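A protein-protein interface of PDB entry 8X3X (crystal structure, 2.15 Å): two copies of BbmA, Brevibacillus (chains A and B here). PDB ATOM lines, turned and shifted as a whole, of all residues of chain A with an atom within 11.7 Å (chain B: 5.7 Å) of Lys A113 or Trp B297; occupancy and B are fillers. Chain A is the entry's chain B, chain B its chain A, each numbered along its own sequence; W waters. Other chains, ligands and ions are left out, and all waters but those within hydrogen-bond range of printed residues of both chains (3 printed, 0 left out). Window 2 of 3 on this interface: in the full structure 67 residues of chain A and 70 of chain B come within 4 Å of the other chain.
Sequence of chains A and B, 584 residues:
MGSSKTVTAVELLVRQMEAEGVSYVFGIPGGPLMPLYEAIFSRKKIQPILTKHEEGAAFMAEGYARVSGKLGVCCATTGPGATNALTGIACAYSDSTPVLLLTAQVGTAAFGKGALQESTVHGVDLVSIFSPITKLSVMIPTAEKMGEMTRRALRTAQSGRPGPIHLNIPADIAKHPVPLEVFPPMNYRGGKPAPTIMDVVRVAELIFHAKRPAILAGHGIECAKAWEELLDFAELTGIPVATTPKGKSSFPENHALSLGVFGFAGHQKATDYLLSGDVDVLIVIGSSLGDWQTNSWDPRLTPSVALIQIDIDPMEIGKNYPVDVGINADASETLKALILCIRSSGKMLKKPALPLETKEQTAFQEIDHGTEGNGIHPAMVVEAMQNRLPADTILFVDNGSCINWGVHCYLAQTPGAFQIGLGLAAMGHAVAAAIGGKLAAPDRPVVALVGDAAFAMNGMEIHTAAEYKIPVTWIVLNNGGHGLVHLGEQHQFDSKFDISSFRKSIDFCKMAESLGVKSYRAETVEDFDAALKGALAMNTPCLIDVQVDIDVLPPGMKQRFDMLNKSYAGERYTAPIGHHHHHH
The side-chain amide nitrogen (ND2) of Asn B320 lies within hydrogen-bond range of the backbone carbonyl oxygen (O) of Lys A113 (2.8 Å). N of Asp B291 is in hydrogen-bond range of O of Gly A114, at 3.1 Å. NE1 of Trp B297 lies within hydrogen-bond range of O of Lys A113 (3.2 Å).
OG1 of Thr B294 sits at hydrogen-bond distance from O of Asp B291 (3.5 Å). ND2 of Asn B320 is in hydrogen-bond range of O of Leu B289 (2.8 Å). The backbone carbonyl oxygen (O) of Gly B290 lies within hydrogen-bond range of the side-chain hydroxyl (OG1) of Thr B294 (2.8 Å). The backbone NH (N) of Trp B297 sits at hydrogen-bond distance from the side-chain hydroxyl (OG1) of Thr B294, at 2.7 Å. The indole nitrogen of Trp B297 sits at hydrogen-bond distance from the backbone carbonyl oxygen of Leu B289 (3.1 Å). The side-chain amide nitrogen (ND2) of Asn B320 lies close to the indole nitrogen (NE1) of Trp B297 (3.2 Å).
Lys B319 touches Gly A112 (CD to O, 3.6 Å). O of Leu B289 touches O of Lys A113, at 3.9 Å. O of Lys A113 touches CA of Gly B290, 3.8 Å away. Lys B319 touches Lys A113 (CE to O, 3.8 Å). Gly B290 touches Gly A114. CZ2 of Trp B297 touches O of Gly A114, 3.8 Å away.
Of chain B, only Leu B289 (3.9 Å), Gly B290 (3.8 Å), Trp B297 (3.2 Å), Lys B319 (3.8 Å) and Asn B320 (2.8 Å) come within 4 Å of Lys A113. Of chain A, only Lys A113 and Gly A114 come within 4 Å of Gly B290. Of chain A, only Gly A114 (3.1 Å) comes within 4 Å of Asp B291. No residue of chain A comes within 4 Å of Thr B294. No residue of chain A comes within 4 Å of Asn B295. No residue of chain A comes within 4 Å of Ser B296. Asp B298 touches none of the printed residues of chain A. Pro B299 touches none of the printed residues of chain A. Of the printed residues of chain B, Gly A114 touches Gly B290 (3.5 Å), Asp B291 (3.1 Å) and Trp B297 (3.8 Å). Of the printed residues of chain A, Lys B319 touches Gly A112 (3.6 Å) and Lys A113 (3.8 Å). Printed residues of chain B within 4 Å of Gly A112: Lys B319. Ser A119 touches none of the printed residues of chain B. Gln A117 touches none of the printed residues of chain B. The nearest residue of chain B that does not touch Lys A113 is Asp B291 (4.8 Å). The nearest printed residue of chain B that does not touch Gly A112 is Asn B320 (4.6 Å).
Printed residues of chain B that touch a printed residue of chain A: Leu B289, Gly B290, Asp B291, Trp B297, Lys B319 and Asn B320. Hydrophobic or aromatic side chains of chain B that line the printed part of chain A: Trp B297. Of the 20 printed residues of chain A, 3 touch a printed residue of chain B.
No position is printed for both chains. Of the 9 pairs that touch across the chains among the printed residues, none has its exchanged pair printed and touching as well.
Water W1 bridges the side-chain carboxylate of Asp B291 (2.5 Å) and the backbone NH of Leu A116 (3.1 Å). Water W3 lies within hydrogen-bond range of the side-chain amino group of Lys B319 (2.6 Å), the backbone carbonyl oxygen of Ser B288 (2.9 Å), the backbone carbonyl oxygen of Lys A113 (3.3 Å) and the backbone NH of Gly B290 (3.5 Å). Water W2 lies within hydrogen-bond range of the backbone carbonyl oxygen of Asn B320 and the side-chain amino group of Lys A113.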
ATOM      1  N   GLN A 105     -10.515  -9.447 -24.004  1.00  0.00           N
ATOM      2  CA  GLN A 105     -10.567 -10.772 -24.593  1.00  0.00           C
ATOM      3  C   GLN A 105      -9.354 -11.540 -24.068  1.00  0.00           C
ATOM      4  O   GLN A 105      -8.309 -10.945 -23.784  1.00  0.00           O
ATOM      5  CB  GLN A 105     -10.552 -10.673 -26.135  1.00  0.00           C
ATOM      6  CG  GLN A 105     -10.666 -11.993 -26.858  1.00  0.00           C
ATOM      7  CD  GLN A 105     -11.955 -12.707 -26.518  1.00  0.00           C
ATOM      8  OE1 GLN A 105     -11.982 -13.611 -25.675  1.00  0.00           O
ATOM      9  NE2 GLN A 105     -13.042 -12.292 -27.160  1.00  0.00           N
ATOM     10  N   VAL A 106      -9.486 -12.859 -23.942  1.00  0.00           N
ATOM     11  CA  VAL A 106      -8.359 -13.683 -23.492  1.00  0.00           C
ATOM     12  C   VAL A 106      -7.277 -13.669 -24.564  1.00  0.00           C
ATOM     13  O   VAL A 106      -7.512 -13.225 -25.700  1.00  0.00           O
ATOM     14  CB  VAL A 106      -8.787 -15.131 -23.179  1.00  0.00           C
ATOM     15  CG1 VAL A 106      -9.981 -15.148 -22.197  1.00  0.00           C
ATOM     16  CG2 VAL A 106      -9.125 -15.873 -24.477  1.00  0.00           C
ATOM     17  N   GLY A 107      -6.096 -14.173 -24.216  1.00  0.00           N
ATOM     18  CA  GLY A 107      -5.017 -14.250 -25.187  1.00  0.00           C
ATOM     19  C   GLY A 107      -5.344 -15.203 -26.326  1.00  0.00           C
ATOM     20  O   GLY A 107      -5.998 -16.235 -26.143  1.00  0.00           O
ATOM     21  N   THR A 108      -4.858 -14.845 -27.514  1.00  0.00           N
ATOM     22  CA  THR A 108      -5.086 -15.637 -28.724  1.00  0.00           C
ATOM     23  C   THR A 108      -4.712 -17.104 -28.538  1.00  0.00           C
ATOM     24  O   THR A 108      -5.392 -17.995 -29.060  1.00  0.00           O
ATOM     25  CB  THR A 108      -4.278 -15.045 -29.880  1.00  0.00           C
ATOM     26  OG1 THR A 108      -4.574 -15.768 -31.079  1.00  0.00           O
ATOM     27  CG2 THR A 108      -2.776 -15.156 -29.590  1.00  0.00           C
ATOM     28  N   ALA A 109      -3.626 -17.374 -27.808  1.00  0.00           N
ATOM     29  CA  ALA A 109      -3.127 -18.734 -27.619  1.00  0.00           C
ATOM     30  C   ALA A 109      -4.110 -19.634 -26.880  1.00  0.00           C
ATOM     31  O   ALA A 109      -3.940 -20.859 -26.898  1.00  0.00           O
ATOM     32  CB  ALA A 109      -1.793 -18.696 -26.870  1.00  0.00           C
ATOM     33  N   ALA A 110      -5.128 -19.069 -26.235  1.00  0.00           N
ATOM     34  CA  ALA A 110      -6.075 -19.853 -25.459  1.00  0.00           C
ATOM     35  C   ALA A 110      -7.412 -20.049 -26.173  1.00  0.00           C
ATOM     36  O   ALA A 110      -8.303 -20.708 -25.620  1.00  0.00           O
ATOM     37  CB  ALA A 110      -6.297 -19.186 -24.088  1.00  0.00           C
ATOM     38  N   PHE A 111      -7.582 -19.491 -27.378  1.00  0.00           N
ATOM     39  CA  PHE A 111      -8.856 -19.604 -28.094  1.00  0.00           C
ATOM     40  C   PHE A 111      -9.212 -21.072 -28.307  1.00  0.00           C
ATOM     41  O   PHE A 111      -8.400 -21.854 -28.826  1.00  0.00           O
ATOM     42  CB  PHE A 111      -8.791 -18.909 -29.458  1.00  0.00           C
ATOM     43  CG  PHE A 111      -8.921 -17.400 -29.405  1.00  0.00           C
ATOM     44  CD1 PHE A 111      -8.708 -16.699 -28.219  1.00  0.00           C
ATOM     45  CD2 PHE A 111      -9.224 -16.678 -30.561  1.00  0.00           C
ATOM     46  CE1 PHE A 111      -8.805 -15.311 -28.180  1.00  0.00           C
ATOM     47  CE2 PHE A 111      -9.324 -15.281 -30.530  1.00  0.00           C
ATOM     48  CZ  PHE A 111      -9.105 -14.603 -29.335  1.00  0.00           C
ATOM     49  N   GLY A 112     -10.432 -21.438 -27.910  1.00  0.00           N
ATOM     50  CA  GLY A 112     -10.962 -22.765 -28.133  1.00  0.00           C
ATOM     51  C   GLY A 112     -10.480 -23.824 -27.163  1.00  0.00           C
ATOM     52  O   GLY A 112     -10.750 -25.008 -27.392  1.00  0.00           O
ATOM     53  N   LYS A 113      -9.778 -23.445 -26.086  1.00  0.00           N
ATOM     54  CA  LYS A 113      -9.300 -24.404 -25.097  1.00  0.00           C
ATOM     55  C   LYS A 113     -10.079 -24.355 -23.792  1.00  0.00           C
ATOM     56  O   LYS A 113      -9.829 -25.183 -22.908  1.00  0.00           O
ATOM     57  CB  LYS A 113      -7.812 -24.188 -24.801  1.00  0.00           C
ATOM     58  CG  LYS A 113      -6.925 -24.212 -26.039  1.00  0.00           C
ATOM     59  CD  LYS A 113      -5.449 -24.093 -25.671  1.00  0.00           C
ATOM     60  CE  LYS A 113      -4.960 -25.317 -24.899  1.00  0.00           C
ATOM     61  NZ  LYS A 113      -5.077 -26.566 -25.725  1.00  0.00           N
ATOM     62  N   GLY A 114     -11.012 -23.424 -23.643  1.00  0.00           N
ATOM     63  CA  GLY A 114     -11.705 -23.266 -22.373  1.00  0.00           C
ATOM     64  C   GLY A 114     -11.024 -22.248 -21.473  1.00  0.00           C
ATOM     65  O   GLY A 114     -10.856 -22.472 -20.269  1.00  0.00           O
ATOM     66  N   ALA A 115     -10.638 -21.110 -22.052  1.00  0.00           N
ATOM     67  CA  ALA A 115     -10.013 -20.046 -21.275  1.00  0.00           C
ATOM     68  C   ALA A 115     -10.976 -19.469 -20.238  1.00  0.00           C
ATOM     69  O   ALA A 115     -12.206 -19.522 -20.374  1.00  0.00           O
ATOM     70  CB  ALA A 115      -9.515 -18.928 -22.191  1.00  0.00           C
ATOM     71  N   LEU A 116     -10.394 -18.909 -19.184  1.00  0.00           N
ATOM     72  CA  LEU A 116     -11.181 -18.262 -18.145  1.00  0.00           C
ATOM     73  C   LEU A 116     -12.009 -17.140 -18.762  1.00  0.00           C
ATOM     74  O   LEU A 116     -11.463 -16.240 -19.400  1.00  0.00           O
ATOM     75  CB  LEU A 116     -10.256 -17.720 -17.051  1.00  0.00           C
ATOM     76  CG  LEU A 116     -10.929 -16.828 -16.005  1.00  0.00           C
ATOM     77  CD1 LEU A 116     -11.979 -17.617 -15.226  1.00  0.00           C
ATOM     78  CD2 LEU A 116      -9.908 -16.197 -15.059  1.00  0.00           C
ATOM     79  N   GLN A 117     -13.328 -17.213 -18.594  1.00  0.00           N
ATOM     80  CA  GLN A 117     -14.247 -16.233 -19.168  1.00  0.00           C
ATOM     81  C   GLN A 117     -14.026 -16.072 -20.672  1.00  0.00           C
ATOM     82  O   GLN A 117     -14.223 -14.986 -21.232  1.00  0.00           O
ATOM     83  CB  GLN A 117     -14.133 -14.890 -18.434  1.00  0.00           C
ATOM     84  CG  GLN A 117     -14.483 -14.995 -16.928  1.00  0.00           C
ATOM     85  CD  GLN A 117     -14.312 -13.684 -16.172  1.00  0.00           C
ATOM     86  OE1 GLN A 117     -13.551 -12.821 -16.590  1.00  0.00           O
ATOM     87  NE2 GLN A 117     -15.011 -13.541 -15.041  1.00  0.00           N
ATOM     88  N   GLU A 118     -13.648 -17.162 -21.353  1.00  0.00           N
ATOM     89  CA  GLU A 118     -13.398 -17.069 -22.791  1.00  0.00           C
ATOM     90  C   GLU A 118     -14.572 -16.383 -23.479  1.00  0.00           C
ATOM     91  O   GLU A 118     -15.737 -16.726 -23.249  1.00  0.00           O
ATOM     92  CB  GLU A 118     -13.152 -18.448 -23.416  1.00  0.00           C
ATOM     93  CG  GLU A 118     -12.661 -18.318 -24.883  1.00  0.00           C
ATOM     94  CD  GLU A 118     -12.191 -19.630 -25.524  1.00  0.00           C
ATOM     95  OE1 GLU A 118     -12.144 -19.689 -26.771  1.00  0.00           O
ATOM     96  OE2 GLU A 118     -11.864 -20.597 -24.797  1.00  0.00           O
ATOM     97  N   SER A 119     -14.260 -15.402 -24.313  1.00  0.00           N
ATOM     98  CA  SER A 119     -15.277 -14.524 -24.884  1.00  0.00           C
ATOM     99  C   SER A 119     -15.263 -14.549 -26.405  1.00  0.00           C
ATOM    100  O   SER A 119     -15.586 -13.555 -27.065  1.00  0.00           O
ATOM    101  CB  SER A 119     -15.108 -13.108 -24.344  1.00  0.00           C
ATOM    102  OG  SER A 119     -15.235 -13.127 -22.925  1.00  0.00           O
ATOM    103  N   THR A 120     -14.901 -15.698 -26.955  1.00  0.00           N
ATOM    104  CA  THR A 120     -14.909 -15.998 -28.373  1.00  0.00           C
ATOM    105  C   THR A 120     -16.168 -16.768 -28.749  1.00  0.00           C
ATOM    106  O   THR A 120     -17.014 -17.088 -27.908  1.00  0.00           O
ATOM    107  CB  THR A 120     -13.702 -16.853 -28.718  1.00  0.00           C
ATOM    108  OG1 THR A 120     -13.873 -18.121 -28.060  1.00  0.00           O
ATOM    109  CG2 THR A 120     -12.402 -16.185 -28.227  1.00  0.00           C
ATOM    110  N   VAL A 121     -16.243 -17.139 -30.033  1.00  0.00           N
ATOM    111  CA  VAL A 121     -17.318 -18.003 -30.510  1.00  0.00           C
ATOM    112  C   VAL A 121     -17.319 -19.330 -29.756  1.00  0.00           C
ATOM    113  O   VAL A 121     -18.376 -19.964 -29.597  1.00  0.00           O
ATOM    114  CB  VAL A 121     -17.183 -18.205 -32.034  1.00  0.00           C
ATOM    115  CG1 VAL A 121     -15.874 -18.932 -32.372  1.00  0.00           C
ATOM    116  CG2 VAL A 121     -18.420 -18.931 -32.615  1.00  0.00           C
ATOM    117  N   HIS A 122     -16.153 -19.762 -29.251  1.00  0.00           N
ATOM    118  CA  HIS A 122     -16.091 -21.021 -28.515  1.00  0.00           C
ATOM    119  C   HIS A 122     -16.534 -20.884 -27.062  1.00  0.00           C
ATOM    120  O   HIS A 122     -16.652 -21.901 -26.367  1.00  0.00           O
ATOM    121  CB  HIS A 122     -14.668 -21.606 -28.554  1.00  0.00           C
ATOM    122  CG  HIS A 122     -14.013 -21.567 -29.908  1.00  0.00           C
ATOM    123  ND1 HIS A 122     -14.373 -22.414 -30.939  1.00  0.00           N
ATOM    124  CD2 HIS A 122     -13.003 -20.798 -30.386  1.00  0.00           C
ATOM    125  CE1 HIS A 122     -13.613 -22.165 -31.993  1.00  0.00           C
ATOM    126  NE2 HIS A 122     -12.778 -21.185 -31.687  1.00  0.00           N
ATOM    127  N   GLY A 123     -16.768 -19.670 -26.579  1.00  0.00           N
ATOM    128  CA  GLY A 123     -17.208 -19.484 -25.212  1.00  0.00           C
ATOM    129  C   GLY A 123     -18.439 -18.608 -25.150  1.00  0.00           C
ATOM    130  O   GLY A 123     -19.504 -18.995 -25.630  1.00  0.00           O
ATOM    131  N   VAL A 124     -18.289 -17.408 -24.594  1.00  0.00           N
ATOM    132  CA  VAL A 124     -19.348 -16.405 -24.537  1.00  0.00           C
ATOM    133  C   VAL A 124     -18.985 -15.342 -25.570  1.00  0.00           C
ATOM    134  O   VAL A 124     -18.091 -14.513 -25.348  1.00  0.00           O
ATOM    135  CB  VAL A 124     -19.490 -15.833 -23.124  1.00  0.00           C
ATOM    136  CG1 VAL A 124     -20.389 -14.606 -23.109  1.00  0.00           C
ATOM    137  CG2 VAL A 124     -20.030 -16.928 -22.175  1.00  0.00           C
ATOM    138  N   SER B 288     -14.816 -30.260 -18.650  1.00  0.00           N
ATOM    139  CA  SER B 288     -14.419 -29.685 -19.931  1.00  0.00           C
ATOM    140  C   SER B 288     -12.913 -29.473 -20.045  1.00  0.00           C
ATOM    141  O   SER B 288     -12.439 -29.104 -21.122  1.00  0.00           O
ATOM    142  CB  SER B 288     -15.150 -28.351 -20.179  1.00  0.00           C
ATOM    143  OG  SER B 288     -14.845 -27.374 -19.184  1.00  0.00           O
ATOM    144  N   LEU B 289     -12.158 -29.685 -18.970  1.00  0.00           N
ATOM    145  CA  LEU B 289     -10.701 -29.546 -18.987  1.00  0.00           C
ATOM    146  C   LEU B 289     -10.281 -28.169 -19.504  1.00  0.00           C
ATOM    147  O   LEU B 289      -9.359 -28.023 -20.316  1.00  0.00           O
ATOM    148  CB  LEU B 289     -10.050 -30.681 -19.790  1.00  0.00           C
ATOM    149  CG  LEU B 289     -10.292 -32.083 -19.192  1.00  0.00           C
ATOM    150  CD1 LEU B 289      -9.641 -33.210 -20.018  1.00  0.00           C
ATOM    151  CD2 LEU B 289      -9.794 -32.142 -17.738  1.00  0.00           C
ATOM    152  N   GLY B 290     -10.948 -27.140 -18.988  1.00  0.00           N
ATOM    153  CA  GLY B 290     -10.530 -25.771 -19.217  1.00  0.00           C
ATOM    154  C   GLY B 290      -9.315 -25.378 -18.377  1.00  0.00           C
ATOM    155  O   GLY B 290      -8.637 -26.206 -17.764  1.00  0.00           O
ATOM    156  N   ASP B 291      -9.074 -24.058 -18.336  1.00  0.00           N
ATOM    157  CA  ASP B 291      -7.848 -23.491 -17.765  1.00  0.00           C
ATOM    158  C   ASP B 291      -7.676 -23.869 -16.298  1.00  0.00           C
ATOM    159  O   ASP B 291      -6.674 -24.477 -15.905  1.00  0.00           O
ATOM    160  CB  ASP B 291      -7.870 -21.965 -17.927  1.00  0.00           C
ATOM    161  CG  ASP B 291      -6.601 -21.280 -17.378  1.00  0.00           C
ATOM    162  OD1 ASP B 291      -5.752 -21.946 -16.757  1.00  0.00           O
ATOM    163  OD2 ASP B 291      -6.461 -20.054 -17.579  1.00  0.00           O
ATOM    164  N   THR B 294      -6.975 -27.550 -15.270  1.00  0.00           N
ATOM    165  CA  THR B 294      -5.795 -28.261 -15.751  1.00  0.00           C
ATOM    166  C   THR B 294      -4.509 -27.510 -15.450  1.00  0.00           C
ATOM    167  O   THR B 294      -3.459 -27.849 -16.021  1.00  0.00           O
ATOM    168  CB  THR B 294      -5.895 -28.501 -17.262  1.00  0.00           C
ATOM    169  OG1 THR B 294      -5.985 -27.229 -17.920  1.00  0.00           O
ATOM    170  CG2 THR B 294      -7.152 -29.323 -17.604  1.00  0.00           C
ATOM    171  N   ASN B 295      -4.566 -26.484 -14.603  1.00  0.00           N
ATOM    172  CA  ASN B 295      -3.411 -25.616 -14.377  1.00  0.00           C
ATOM    173  C   ASN B 295      -2.880 -25.088 -15.702  1.00  0.00           C
ATOM    174  O   ASN B 295      -1.699 -25.220 -16.031  1.00  0.00           O
ATOM    175  CB  ASN B 295      -2.330 -26.351 -13.598  1.00  0.00           C
ATOM    176  CG  ASN B 295      -2.670 -26.452 -12.125  1.00  0.00           C
ATOM    177  OD1 ASN B 295      -3.462 -25.654 -11.610  1.00  0.00           O
ATOM    178  ND2 ASN B 295      -2.094 -27.441 -11.439  1.00  0.00           N
ATOM    179  N   SER B 296      -3.784 -24.507 -16.488  1.00  0.00           N
ATOM    180  CA  SER B 296      -3.427 -23.942 -17.780  1.00  0.00           C
ATOM    181  C   SER B 296      -2.917 -25.023 -18.739  1.00  0.00           C
ATOM    182  O   SER B 296      -1.890 -24.863 -19.395  1.00  0.00           O
ATOM    183  CB  SER B 296      -2.393 -22.826 -17.601  1.00  0.00           C
ATOM    184  OG  SER B 296      -2.451 -21.917 -18.679  1.00  0.00           O
ATOM    185  N   TRP B 297      -3.645 -26.145 -18.812  1.00  0.00           N
ATOM    186  CA  TRP B 297      -3.333 -27.218 -19.763  1.00  0.00           C
ATOM    187  C   TRP B 297      -1.910 -27.747 -19.568  1.00  0.00           C
ATOM    188  O   TRP B 297      -1.141 -27.935 -20.517  1.00  0.00           O
ATOM    189  CB  TRP B 297      -3.578 -26.730 -21.194  1.00  0.00           C
ATOM    190  CG  TRP B 297      -4.951 -26.138 -21.263  1.00  0.00           C
ATOM    191  CD1 TRP B 297      -6.142 -26.825 -21.200  1.00  0.00           C
ATOM    192  CD2 TRP B 297      -5.297 -24.746 -21.314  1.00  0.00           C
ATOM    193  NE1 TRP B 297      -7.192 -25.951 -21.238  1.00  0.00           N
ATOM    194  CE2 TRP B 297      -6.708 -24.669 -21.314  1.00  0.00           C
ATOM    195  CE3 TRP B 297      -4.554 -23.558 -21.385  1.00  0.00           C
ATOM    196  CZ2 TRP B 297      -7.393 -23.453 -21.380  1.00  0.00           C
ATOM    197  CZ3 TRP B 297      -5.238 -22.348 -21.454  1.00  0.00           C
ATOM    198  CH2 TRP B 297      -6.639 -22.307 -21.446  1.00  0.00           C
ATOM    199  N   ASP B 298      -1.572 -28.007 -18.315  1.00  0.00           N
ATOM    200  CA  ASP B 298      -0.269 -28.554 -17.972  1.00  0.00           C
ATOM    201  C   ASP B 298      -0.036 -29.857 -18.734  1.00  0.00           C
ATOM    202  O   ASP B 298      -0.834 -30.789 -18.590  1.00  0.00           O
ATOM    203  CB  ASP B 298      -0.224 -28.790 -16.461  1.00  0.00           C
ATOM    204  CG  ASP B 298       1.173 -29.033 -15.940  1.00  0.00           C
ATOM    205  OD1 ASP B 298       1.952 -29.757 -16.600  1.00  0.00           O
ATOM    206  OD2 ASP B 298       1.480 -28.499 -14.853  1.00  0.00           O
ATOM    207  N   PRO B 299       1.014 -29.966 -19.556  1.00  0.00           N
ATOM    208  CA  PRO B 299       1.235 -31.227 -20.285  1.00  0.00           C
ATOM    209  C   PRO B 299       1.445 -32.425 -19.376  1.00  0.00           C
ATOM    210  O   PRO B 299       1.197 -33.559 -19.810  1.00  0.00           O
ATOM    211  CB  PRO B 299       2.491 -30.946 -21.128  1.00  0.00           C
ATOM    212  CG  PRO B 299       3.073 -29.686 -20.588  1.00  0.00           C
ATOM    213  CD  PRO B 299       1.934 -28.909 -20.003  1.00  0.00           C
ATOM    214  N   LYS B 319     -10.521 -32.611 -26.616  1.00  0.00           N
ATOM    215  CA  LYS B 319     -10.332 -31.220 -27.009  1.00  0.00           C
ATOM    216  C   LYS B 319      -8.920 -30.746 -26.696  1.00  0.00           C
ATOM    217  O   LYS B 319      -8.240 -30.183 -27.561  1.00  0.00           O
ATOM    218  CB  LYS B 319     -11.351 -30.317 -26.309  1.00  0.00           C
ATOM    219  CG  LYS B 319     -11.191 -28.827 -26.676  1.00  0.00           C
ATOM    220  CD  LYS B 319     -12.378 -28.001 -26.154  1.00  0.00           C
ATOM    221  CE  LYS B 319     -12.178 -27.568 -24.731  1.00  0.00           C
ATOM    222  NZ  LYS B 319     -13.495 -27.371 -24.049  1.00  0.00           N
ATOM    223  N   ASN B 320      -8.470 -30.937 -25.450  1.00  0.00           N
ATOM    224  CA  ASN B 320      -7.179 -30.418 -25.004  1.00  0.00           C
ATOM    225  C   ASN B 320      -6.136 -31.488 -24.741  1.00  0.00           C
ATOM    226  O   ASN B 320      -4.950 -31.158 -24.709  1.00  0.00           O
ATOM    227  CB  ASN B 320      -7.351 -29.581 -23.725  1.00  0.00           C
ATOM    228  CG  ASN B 320      -8.043 -28.256 -23.995  1.00  0.00           C
ATOM    229  OD1 ASN B 320      -7.759 -27.607 -24.995  1.00  0.00           O
ATOM    230  ND2 ASN B 320      -8.952 -27.854 -23.113  1.00  0.00           N
ATOM    231  N   TYR B 321      -6.542 -32.745 -24.549  1.00  0.00           N
ATOM    232  CA  TYR B 321      -5.636 -33.854 -24.300  1.00  0.00           C
ATOM    233  C   TYR B 321      -6.054 -35.049 -25.155  1.00  0.00           C
ATOM    234  O   TYR B 321      -7.256 -35.322 -25.297  1.00  0.00           O
ATOM    235  CB  TYR B 321      -5.631 -34.251 -22.812  1.00  0.00           C
ATOM    236  CG  TYR B 321      -5.058 -33.187 -21.880  1.00  0.00           C
ATOM    237  CD1 TYR B 321      -5.872 -32.212 -21.319  1.00  0.00           C
ATOM    238  CD2 TYR B 321      -3.699 -33.171 -21.562  1.00  0.00           C
ATOM    239  CE1 TYR B 321      -5.356 -31.241 -20.462  1.00  0.00           C
ATOM    240  CE2 TYR B 321      -3.172 -32.215 -20.699  1.00  0.00           C
ATOM    241  CZ  TYR B 321      -4.004 -31.244 -20.165  1.00  0.00           C
ATOM    242  OH  TYR B 321      -3.493 -30.287 -19.321  1.00  0.00           O
HETATM  243  O   HOH W   1      -7.282 -18.503 -19.379  1.00  0.00           O
HETATM  244  O   HOH W   2      -3.590 -28.702 -24.362  1.00  0.00           O
HETATM  245  O   HOH W   3     -12.764 -26.291 -21.801  1.00  0.00           O
